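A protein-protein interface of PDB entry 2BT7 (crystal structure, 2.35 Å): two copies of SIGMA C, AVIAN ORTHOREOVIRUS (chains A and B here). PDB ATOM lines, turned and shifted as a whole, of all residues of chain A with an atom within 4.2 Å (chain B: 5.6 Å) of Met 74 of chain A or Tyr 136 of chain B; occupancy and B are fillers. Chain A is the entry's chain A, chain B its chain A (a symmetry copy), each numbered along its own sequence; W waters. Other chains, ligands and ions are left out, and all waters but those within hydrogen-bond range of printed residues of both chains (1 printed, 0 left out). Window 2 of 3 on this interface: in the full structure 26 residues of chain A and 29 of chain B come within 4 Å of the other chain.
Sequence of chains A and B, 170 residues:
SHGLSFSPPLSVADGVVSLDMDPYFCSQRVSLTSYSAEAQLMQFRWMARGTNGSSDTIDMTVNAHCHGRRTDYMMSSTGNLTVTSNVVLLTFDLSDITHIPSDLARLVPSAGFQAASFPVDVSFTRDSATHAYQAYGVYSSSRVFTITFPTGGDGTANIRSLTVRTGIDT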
ATOM      1  N   LEU A  41       3.328   1.444 -22.031  1.00  0.00           N
ATOM      2  CA  LEU A  41       3.844   2.735 -21.620  1.00  0.00           C
ATOM      3  C   LEU A  41       2.768   3.416 -20.797  1.00  0.00           C
ATOM      4  O   LEU A  41       1.766   3.888 -21.323  1.00  0.00           O
ATOM      5  CB  LEU A  41       4.272   3.586 -22.816  1.00  0.00           C
ATOM      6  CG  LEU A  41       5.018   4.887 -22.474  1.00  0.00           C
ATOM      7  CD1 LEU A  41       6.479   4.596 -22.036  1.00  0.00           C
ATOM      8  CD2 LEU A  41       5.000   5.852 -23.659  1.00  0.00           C
ATOM      9  N   THR A  61       5.490  13.988 -13.333  1.00  0.00           N
ATOM     10  CA  THR A  61       4.860  13.359 -14.500  1.00  0.00           C
ATOM     11  C   THR A  61       5.736  12.151 -14.800  1.00  0.00           C
ATOM     12  O   THR A  61       6.957  12.283 -15.030  1.00  0.00           O
ATOM     13  CB  THR A  61       4.858  14.323 -15.710  1.00  0.00           C
ATOM     14  OG1 THR A  61       4.051  15.467 -15.406  1.00  0.00           O
ATOM     15  CG2 THR A  61       4.319  13.665 -16.984  1.00  0.00           C
ATOM     16  N   VAL A  62       5.114  10.973 -14.767  1.00  0.00           N
ATOM     17  CA  VAL A  62       5.838   9.709 -14.844  1.00  0.00           C
ATOM     18  C   VAL A  62       5.406   8.956 -16.087  1.00  0.00           C
ATOM     19  O   VAL A  62       4.217   8.870 -16.408  1.00  0.00           O
ATOM     20  CB  VAL A  62       5.629   8.866 -13.567  1.00  0.00           C
ATOM     21  CG1 VAL A  62       6.439   7.537 -13.613  1.00  0.00           C
ATOM     22  CG2 VAL A  62       6.012   9.688 -12.330  1.00  0.00           C
ATOM     23  N   ASN A  63       6.402   8.494 -16.819  1.00  0.00           N
ATOM     24  CA  ASN A  63       6.227   7.545 -17.883  1.00  0.00           C
ATOM     25  C   ASN A  63       6.889   6.245 -17.408  1.00  0.00           C
ATOM     26  O   ASN A  63       8.106   6.220 -17.145  1.00  0.00           O
ATOM     27  CB  ASN A  63       6.874   8.053 -19.172  1.00  0.00           C
ATOM     28  CG  ASN A  63       5.982   9.027 -19.923  1.00  0.00           C
ATOM     29  OD1 ASN A  63       5.349   8.655 -20.908  1.00  0.00           O
ATOM     30  ND2 ASN A  63       5.918  10.273 -19.459  1.00  0.00           N
ATOM     31  N   HIS A  65       7.663   2.599 -18.535  1.00  0.00           N
ATOM     32  CA  HIS A  65       7.719   1.671 -19.658  1.00  0.00           C
ATOM     33  C   HIS A  65       7.890   0.218 -19.152  1.00  0.00           C
ATOM     34  O   HIS A  65       8.956  -0.168 -18.637  1.00  0.00           O
ATOM     35  CB  HIS A  65       8.859   2.036 -20.589  1.00  0.00           C
ATOM     36  CG  HIS A  65       8.964   1.167 -21.801  1.00  0.00           C
ATOM     37  ND1 HIS A  65      10.139   0.552 -22.172  1.00  0.00           N
ATOM     38  CD2 HIS A  65       8.049   0.835 -22.751  1.00  0.00           C
ATOM     39  CE1 HIS A  65       9.957  -0.099 -23.310  1.00  0.00           C
ATOM     40  NE2 HIS A  65       8.690   0.036 -23.671  1.00  0.00           N
ATOM     41  N   ASP A  72      10.830   0.601 -16.410  1.00  0.00           N
ATOM     42  CA  ASP A  72      11.713   1.774 -16.464  1.00  0.00           C
ATOM     43  C   ASP A  72      10.953   3.080 -16.239  1.00  0.00           C
ATOM     44  O   ASP A  72       9.939   3.342 -16.887  1.00  0.00           O
ATOM     45  CB  ASP A  72      12.429   1.805 -17.798  1.00  0.00           C
ATOM     46  CG  ASP A  72      13.394   0.677 -17.932  1.00  0.00           C
ATOM     47  OD1 ASP A  72      14.079   0.406 -16.925  1.00  0.00           O
ATOM     48  OD2 ASP A  72      13.461   0.055 -19.017  1.00  0.00           O
ATOM     49  N   TYR A  73      11.454   3.887 -15.308  1.00  0.00           N
ATOM     50  CA  TYR A  73      10.793   5.124 -14.880  1.00  0.00           C
ATOM     51  C   TYR A  73      11.476   6.387 -15.451  1.00  0.00           C
ATOM     52  O   TYR A  73      12.677   6.588 -15.261  1.00  0.00           O
ATOM     53  CB  TYR A  73      10.848   5.227 -13.361  1.00  0.00           C
ATOM     54  CG  TYR A  73       9.870   4.399 -12.566  1.00  0.00           C
ATOM     55  CD1 TYR A  73       8.542   4.223 -12.975  1.00  0.00           C
ATOM     56  CD2 TYR A  73      10.260   3.851 -11.353  1.00  0.00           C
ATOM     57  CE1 TYR A  73       7.637   3.470 -12.193  1.00  0.00           C
ATOM     58  CE2 TYR A  73       9.381   3.135 -10.569  1.00  0.00           C
ATOM     59  CZ  TYR A  73       8.076   2.924 -10.990  1.00  0.00           C
ATOM     60  OH  TYR A  73       7.234   2.202 -10.147  1.00  0.00           O
ATOM     61  N   MET A  74      10.690   7.203 -16.156  1.00  0.00           N
ATOM     62  CA  MET A  74      11.088   8.513 -16.672  1.00  0.00           C
ATOM     63  C   MET A  74      10.184   9.570 -16.029  1.00  0.00           C
ATOM     64  O   MET A  74       9.030   9.697 -16.424  1.00  0.00           O
ATOM     65  CB  MET A  74      10.886   8.578 -18.189  1.00  0.00           C
ATOM     66  CG  MET A  74      11.929   7.833 -19.054  1.00  0.00           C
ATOM     67  SD  MET A  74      11.788   6.007 -19.247  1.00  0.00           S
ATOM     68  CE  MET A  74      10.015   5.765 -19.484  1.00  0.00           C
ATOM     69  N   MET A  75      10.700  10.322 -15.055  1.00  0.00           N
ATOM     70  CA  MET A  75       9.894  11.308 -14.342  1.00  0.00           C
ATOM     71  C   MET A  75      10.402  12.721 -14.550  1.00  0.00           C
ATOM     72  O   MET A  75      11.615  12.966 -14.578  1.00  0.00           O
ATOM     73  CB  MET A  75       9.876  11.052 -12.848  1.00  0.00           C
ATOM     74  CG  MET A  75      10.040   9.604 -12.416  1.00  0.00           C
ATOM     75  SD  MET A  75       9.505   9.500 -10.723  1.00  0.00           S
ATOM     76  CE  MET A  75       9.847   7.778 -10.389  1.00  0.00           C
ATOM     77  N   VAL A 164      13.868  12.445 -12.763  1.00  0.00           N
ATOM     78  CA  VAL A 164      14.254  11.180 -12.138  1.00  0.00           C
ATOM     79  C   VAL A 164      14.165  10.086 -13.205  1.00  0.00           C
ATOM     80  O   VAL A 164      13.163   9.975 -13.940  1.00  0.00           O
ATOM     81  CB  VAL A 164      13.410  10.851 -10.885  1.00  0.00           C
ATOM     82  CG1 VAL A 164      13.914   9.560 -10.238  1.00  0.00           C
ATOM     83  CG2 VAL A 164      13.451  12.005  -9.878  1.00  0.00           C
ATOM     84  N   SER B 117       4.700   2.146 -27.246  1.00  0.00           N
ATOM     85  CA  SER B 117       5.767   3.133 -27.348  1.00  0.00           C
ATOM     86  C   SER B 117       6.874   2.836 -26.322  1.00  0.00           C
ATOM     87  O   SER B 117       6.620   2.321 -25.239  1.00  0.00           O
ATOM     88  CB  SER B 117       5.226   4.567 -27.177  1.00  0.00           C
ATOM     89  OG  SER B 117       4.128   4.782 -28.065  1.00  0.00           O
ATOM     90  N   PHE B 118       8.105   3.161 -26.693  1.00  0.00           N
ATOM     91  CA  PHE B 118       9.252   2.933 -25.847  1.00  0.00           C
ATOM     92  C   PHE B 118      10.097   4.226 -25.745  1.00  0.00           C
ATOM     93  O   PHE B 118      10.091   5.039 -26.669  1.00  0.00           O
ATOM     94  CB  PHE B 118      10.105   1.783 -26.418  1.00  0.00           C
ATOM     95  CG  PHE B 118      10.397   1.911 -27.899  1.00  0.00           C
ATOM     96  CD1 PHE B 118       9.442   1.538 -28.858  1.00  0.00           C
ATOM     97  CD2 PHE B 118      11.629   2.399 -28.341  1.00  0.00           C
ATOM     98  CE1 PHE B 118       9.724   1.662 -30.239  1.00  0.00           C
ATOM     99  CE2 PHE B 118      11.907   2.514 -29.713  1.00  0.00           C
ATOM    100  CZ  PHE B 118      10.952   2.143 -30.655  1.00  0.00           C
ATOM    101  N   PRO B 119      10.830   4.407 -24.629  1.00  0.00           N
ATOM    102  CA  PRO B 119      11.680   5.610 -24.506  1.00  0.00           C
ATOM    103  C   PRO B 119      12.843   5.685 -25.505  1.00  0.00           C
ATOM    104  O   PRO B 119      13.485   4.674 -25.785  1.00  0.00           O
ATOM    105  CB  PRO B 119      12.149   5.577 -23.036  1.00  0.00           C
ATOM    106  CG  PRO B 119      11.984   4.153 -22.583  1.00  0.00           C
ATOM    107  CD  PRO B 119      10.859   3.564 -23.414  1.00  0.00           C
ATOM    108  N   VAL B 120      13.071   6.880 -26.066  1.00  0.00           N
ATOM    109  CA  VAL B 120      14.227   7.177 -26.958  1.00  0.00           C
ATOM    110  C   VAL B 120      14.916   8.458 -26.451  1.00  0.00           C
ATOM    111  O   VAL B 120      14.274   9.494 -26.298  1.00  0.00           O
ATOM    112  CB  VAL B 120      13.781   7.372 -28.445  1.00  0.00           C
ATOM    113  CG1 VAL B 120      14.961   7.745 -29.362  1.00  0.00           C
ATOM    114  CG2 VAL B 120      13.084   6.146 -28.987  1.00  0.00           C
ATOM    115  N   GLN B 134      13.860  13.523 -23.697  1.00  0.00           N
ATOM    116  CA  GLN B 134      13.344  12.202 -23.450  1.00  0.00           C
ATOM    117  C   GLN B 134      12.237  12.034 -24.463  1.00  0.00           C
ATOM    118  O   GLN B 134      11.144  12.541 -24.264  1.00  0.00           O
ATOM    119  CB  GLN B 134      12.770  12.117 -22.025  1.00  0.00           C
ATOM    120  CG  GLN B 134      11.973  10.814 -21.742  1.00  0.00           C
ATOM    121  CD  GLN B 134      12.704   9.570 -22.237  1.00  0.00           C
ATOM    122  OE1 GLN B 134      13.697   9.145 -21.646  1.00  0.00           O
ATOM    123  NE2 GLN B 134      12.228   9.001 -23.348  1.00  0.00           N
ATOM    124  N   ALA B 135      12.528  11.376 -25.577  1.00  0.00           N
ATOM    125  CA  ALA B 135      11.532  11.197 -26.631  1.00  0.00           C
ATOM    126  C   ALA B 135      10.888   9.770 -26.587  1.00  0.00           C
ATOM    127  O   ALA B 135      11.114   8.994 -25.649  1.00  0.00           O
ATOM    128  CB  ALA B 135      12.175  11.466 -28.001  1.00  0.00           C
ATOM    129  N   TYR B 136      10.109   9.429 -27.610  1.00  0.00           N
ATOM    130  CA  TYR B 136       9.425   8.133 -27.659  1.00  0.00           C
ATOM    131  C   TYR B 136       9.347   7.649 -29.089  1.00  0.00           C
ATOM    132  O   TYR B 136       9.177   8.435 -30.022  1.00  0.00           O
ATOM    133  CB  TYR B 136       8.022   8.210 -26.978  1.00  0.00           C
ATOM    134  CG  TYR B 136       8.183   8.441 -25.503  1.00  0.00           C
ATOM    135  CD1 TYR B 136       8.542   7.384 -24.656  1.00  0.00           C
ATOM    136  CD2 TYR B 136       8.102   9.725 -24.959  1.00  0.00           C
ATOM    137  CE1 TYR B 136       8.779   7.587 -23.300  1.00  0.00           C
ATOM    138  CE2 TYR B 136       8.339   9.949 -23.572  1.00  0.00           C
ATOM    139  CZ  TYR B 136       8.679   8.869 -22.763  1.00  0.00           C
ATOM    140  OH  TYR B 136       8.921   9.049 -21.416  1.00  0.00           O
ATOM    141  N   GLY B 137       9.524   6.347 -29.259  1.00  0.00           N
ATOM    142  CA  GLY B 137       9.272   5.686 -30.531  1.00  0.00           C
ATOM    143  C   GLY B 137       8.091   4.728 -30.426  1.00  0.00           C
ATOM    144  O   GLY B 137       7.628   4.418 -29.328  1.00  0.00           O
ATOM    145  N   VAL B 138       7.611   4.280 -31.580  1.00  0.00           N
ATOM    146  CA  VAL B 138       6.591   3.242 -31.693  1.00  0.00           C
ATOM    147  C   VAL B 138       6.825   2.536 -33.024  1.00  0.00           C
ATOM    148  O   VAL B 138       7.144   3.186 -34.004  1.00  0.00           O
ATOM    149  CB  VAL B 138       5.137   3.821 -31.557  1.00  0.00           C
ATOM    150  CG1 VAL B 138       4.786   4.791 -32.697  1.00  0.00           C
ATOM    151  CG2 VAL B 138       4.094   2.694 -31.416  1.00  0.00           C
ATOM    152  N   THR B 146       9.096   4.822 -35.770  1.00  0.00           N
ATOM    153  CA  THR B 146       9.155   6.263 -35.984  1.00  0.00           C
ATOM    154  C   THR B 146       9.349   6.873 -34.618  1.00  0.00           C
ATOM    155  O   THR B 146       8.622   6.524 -33.700  1.00  0.00           O
ATOM    156  CB  THR B 146       7.848   6.761 -36.660  1.00  0.00           C
ATOM    157  OG1 THR B 146       7.705   6.124 -37.945  1.00  0.00           O
ATOM    158  CG2 THR B 146       7.838   8.310 -36.854  1.00  0.00           C
ATOM    159  N   ILE B 147      10.361   7.732 -34.467  1.00  0.00           N
ATOM    160  CA  ILE B 147      10.518   8.533 -33.236  1.00  0.00           C
ATOM    161  C   ILE B 147       9.908   9.948 -33.386  1.00  0.00           C
ATOM    162  O   ILE B 147       9.826  10.481 -34.485  1.00  0.00           O
ATOM    163  CB  ILE B 147      11.971   8.569 -32.707  1.00  0.00           C
ATOM    164  CG1 ILE B 147      12.857   9.488 -33.562  1.00  0.00           C
ATOM    165  CG2 ILE B 147      12.566   7.164 -32.680  1.00  0.00           C
ATOM    166  CD1 ILE B 147      14.336   9.482 -33.136  1.00  0.00           C
ATOM    167  N   THR B 148       9.446  10.517 -32.278  1.00  0.00           N
ATOM    168  CA  THR B 148       8.766  11.808 -32.274  1.00  0.00           C
ATOM    169  C   THR B 148       9.504  12.650 -31.260  1.00  0.00           C
ATOM    170  O   THR B 148       9.629  12.231 -30.122  1.00  0.00           O
ATOM    171  CB  THR B 148       7.278  11.661 -31.849  1.00  0.00           C
ATOM    172  OG1 THR B 148       6.563  10.906 -32.836  1.00  0.00           O
ATOM    173  CG2 THR B 148       6.568  13.038 -31.658  1.00  0.00           C
HETATM  174  O   HOH W   1       7.403  -0.865 -26.125  1.00  0.00           O
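Of the 10 printed residues of chain A, 4 touch a printed residue of chain B. Hydrophobic or aromatic side chains of chain A that line the printed part of chain B: Leu 41, His 65 and Met 74. Printed residues of chain B that touch a printed residue of chain A: Ser 117, Phe 118, Pro 119, Gln 134 and Tyr 136.
The backbone NH (N) of His 65 of chain A lies within hydrogen-bond range of the backbone carbonyl oxygen (O) of Asp 72 of chain A. The backbone carbonyl oxygen of Met 74 of chain A lies within hydrogen-bond range of the backbone NH of Asn 63 of chain A (2.9 Å). The backbone carbonyl oxygen (O) of Tyr 136 of chain B sits at hydrogen-bond distance from the backbone NH (N) of Thr 148 of chain B, 3.1 Å away. O of Phe 118 of chain B sits at hydrogen-bond distance from N of Gly 137 of chain B (3.0 Å).
Printed residues of chain B within 4 Å of His 65 of chain A: Ser 117 (3.2 Å), Phe 118 (3.5 Å) and Pro 119 (3.3 Å). Of the printed residues of chain A, Phe 118 of chain B touches His 65. Of the printed residues of chain A, Gln 134 of chain B touches Met 74 (3.4 Å). Tyr 136 of chain B touches just these residues of chain A: Leu 41 (3.98 Å), Asn 63 (3.2 Å) and Met 74 (3.8 Å). The nearest printed residue of chain B that does not touch Met 74 of chain A is Phe 118 of chain B (6.4 Å). The nearest printed residue of chain A that does not touch Phe 118 of chain B is Leu 41 of chain A (5.0 Å).
Among the printed residues, pairs that only touch across the chains: Leu 41 of chain A with Ser 117 of chain B, Leu 41 of chain A with Tyr 136 of chain B, Asn 63 of chain A with Tyr 136 of chain B, His 65 of chain A with Phe 118 of chain B, His 65 of chain A with Pro 119 of chain B, Met 74 of chain A with Pro 119 of chain B, Met 74 of chain A with Gln 134 of chain B and Met 74 of chain A with Tyr 136 of chain B.
No position is printed for both chains. Of the 9 pairs that touch across the chains among the printed residues, none has its exchanged pair printed and touching as well.
A ring nitrogen (NE2) of His 65 of chain A lies close to the backbone carbonyl oxygen (O) of Ser 117 of chain B, at 3.5 Å.
Water W1 bridges NE2 of His 65 of chain A (2.9 Å) and O of Ser 117 of chain B (3.4 Å).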
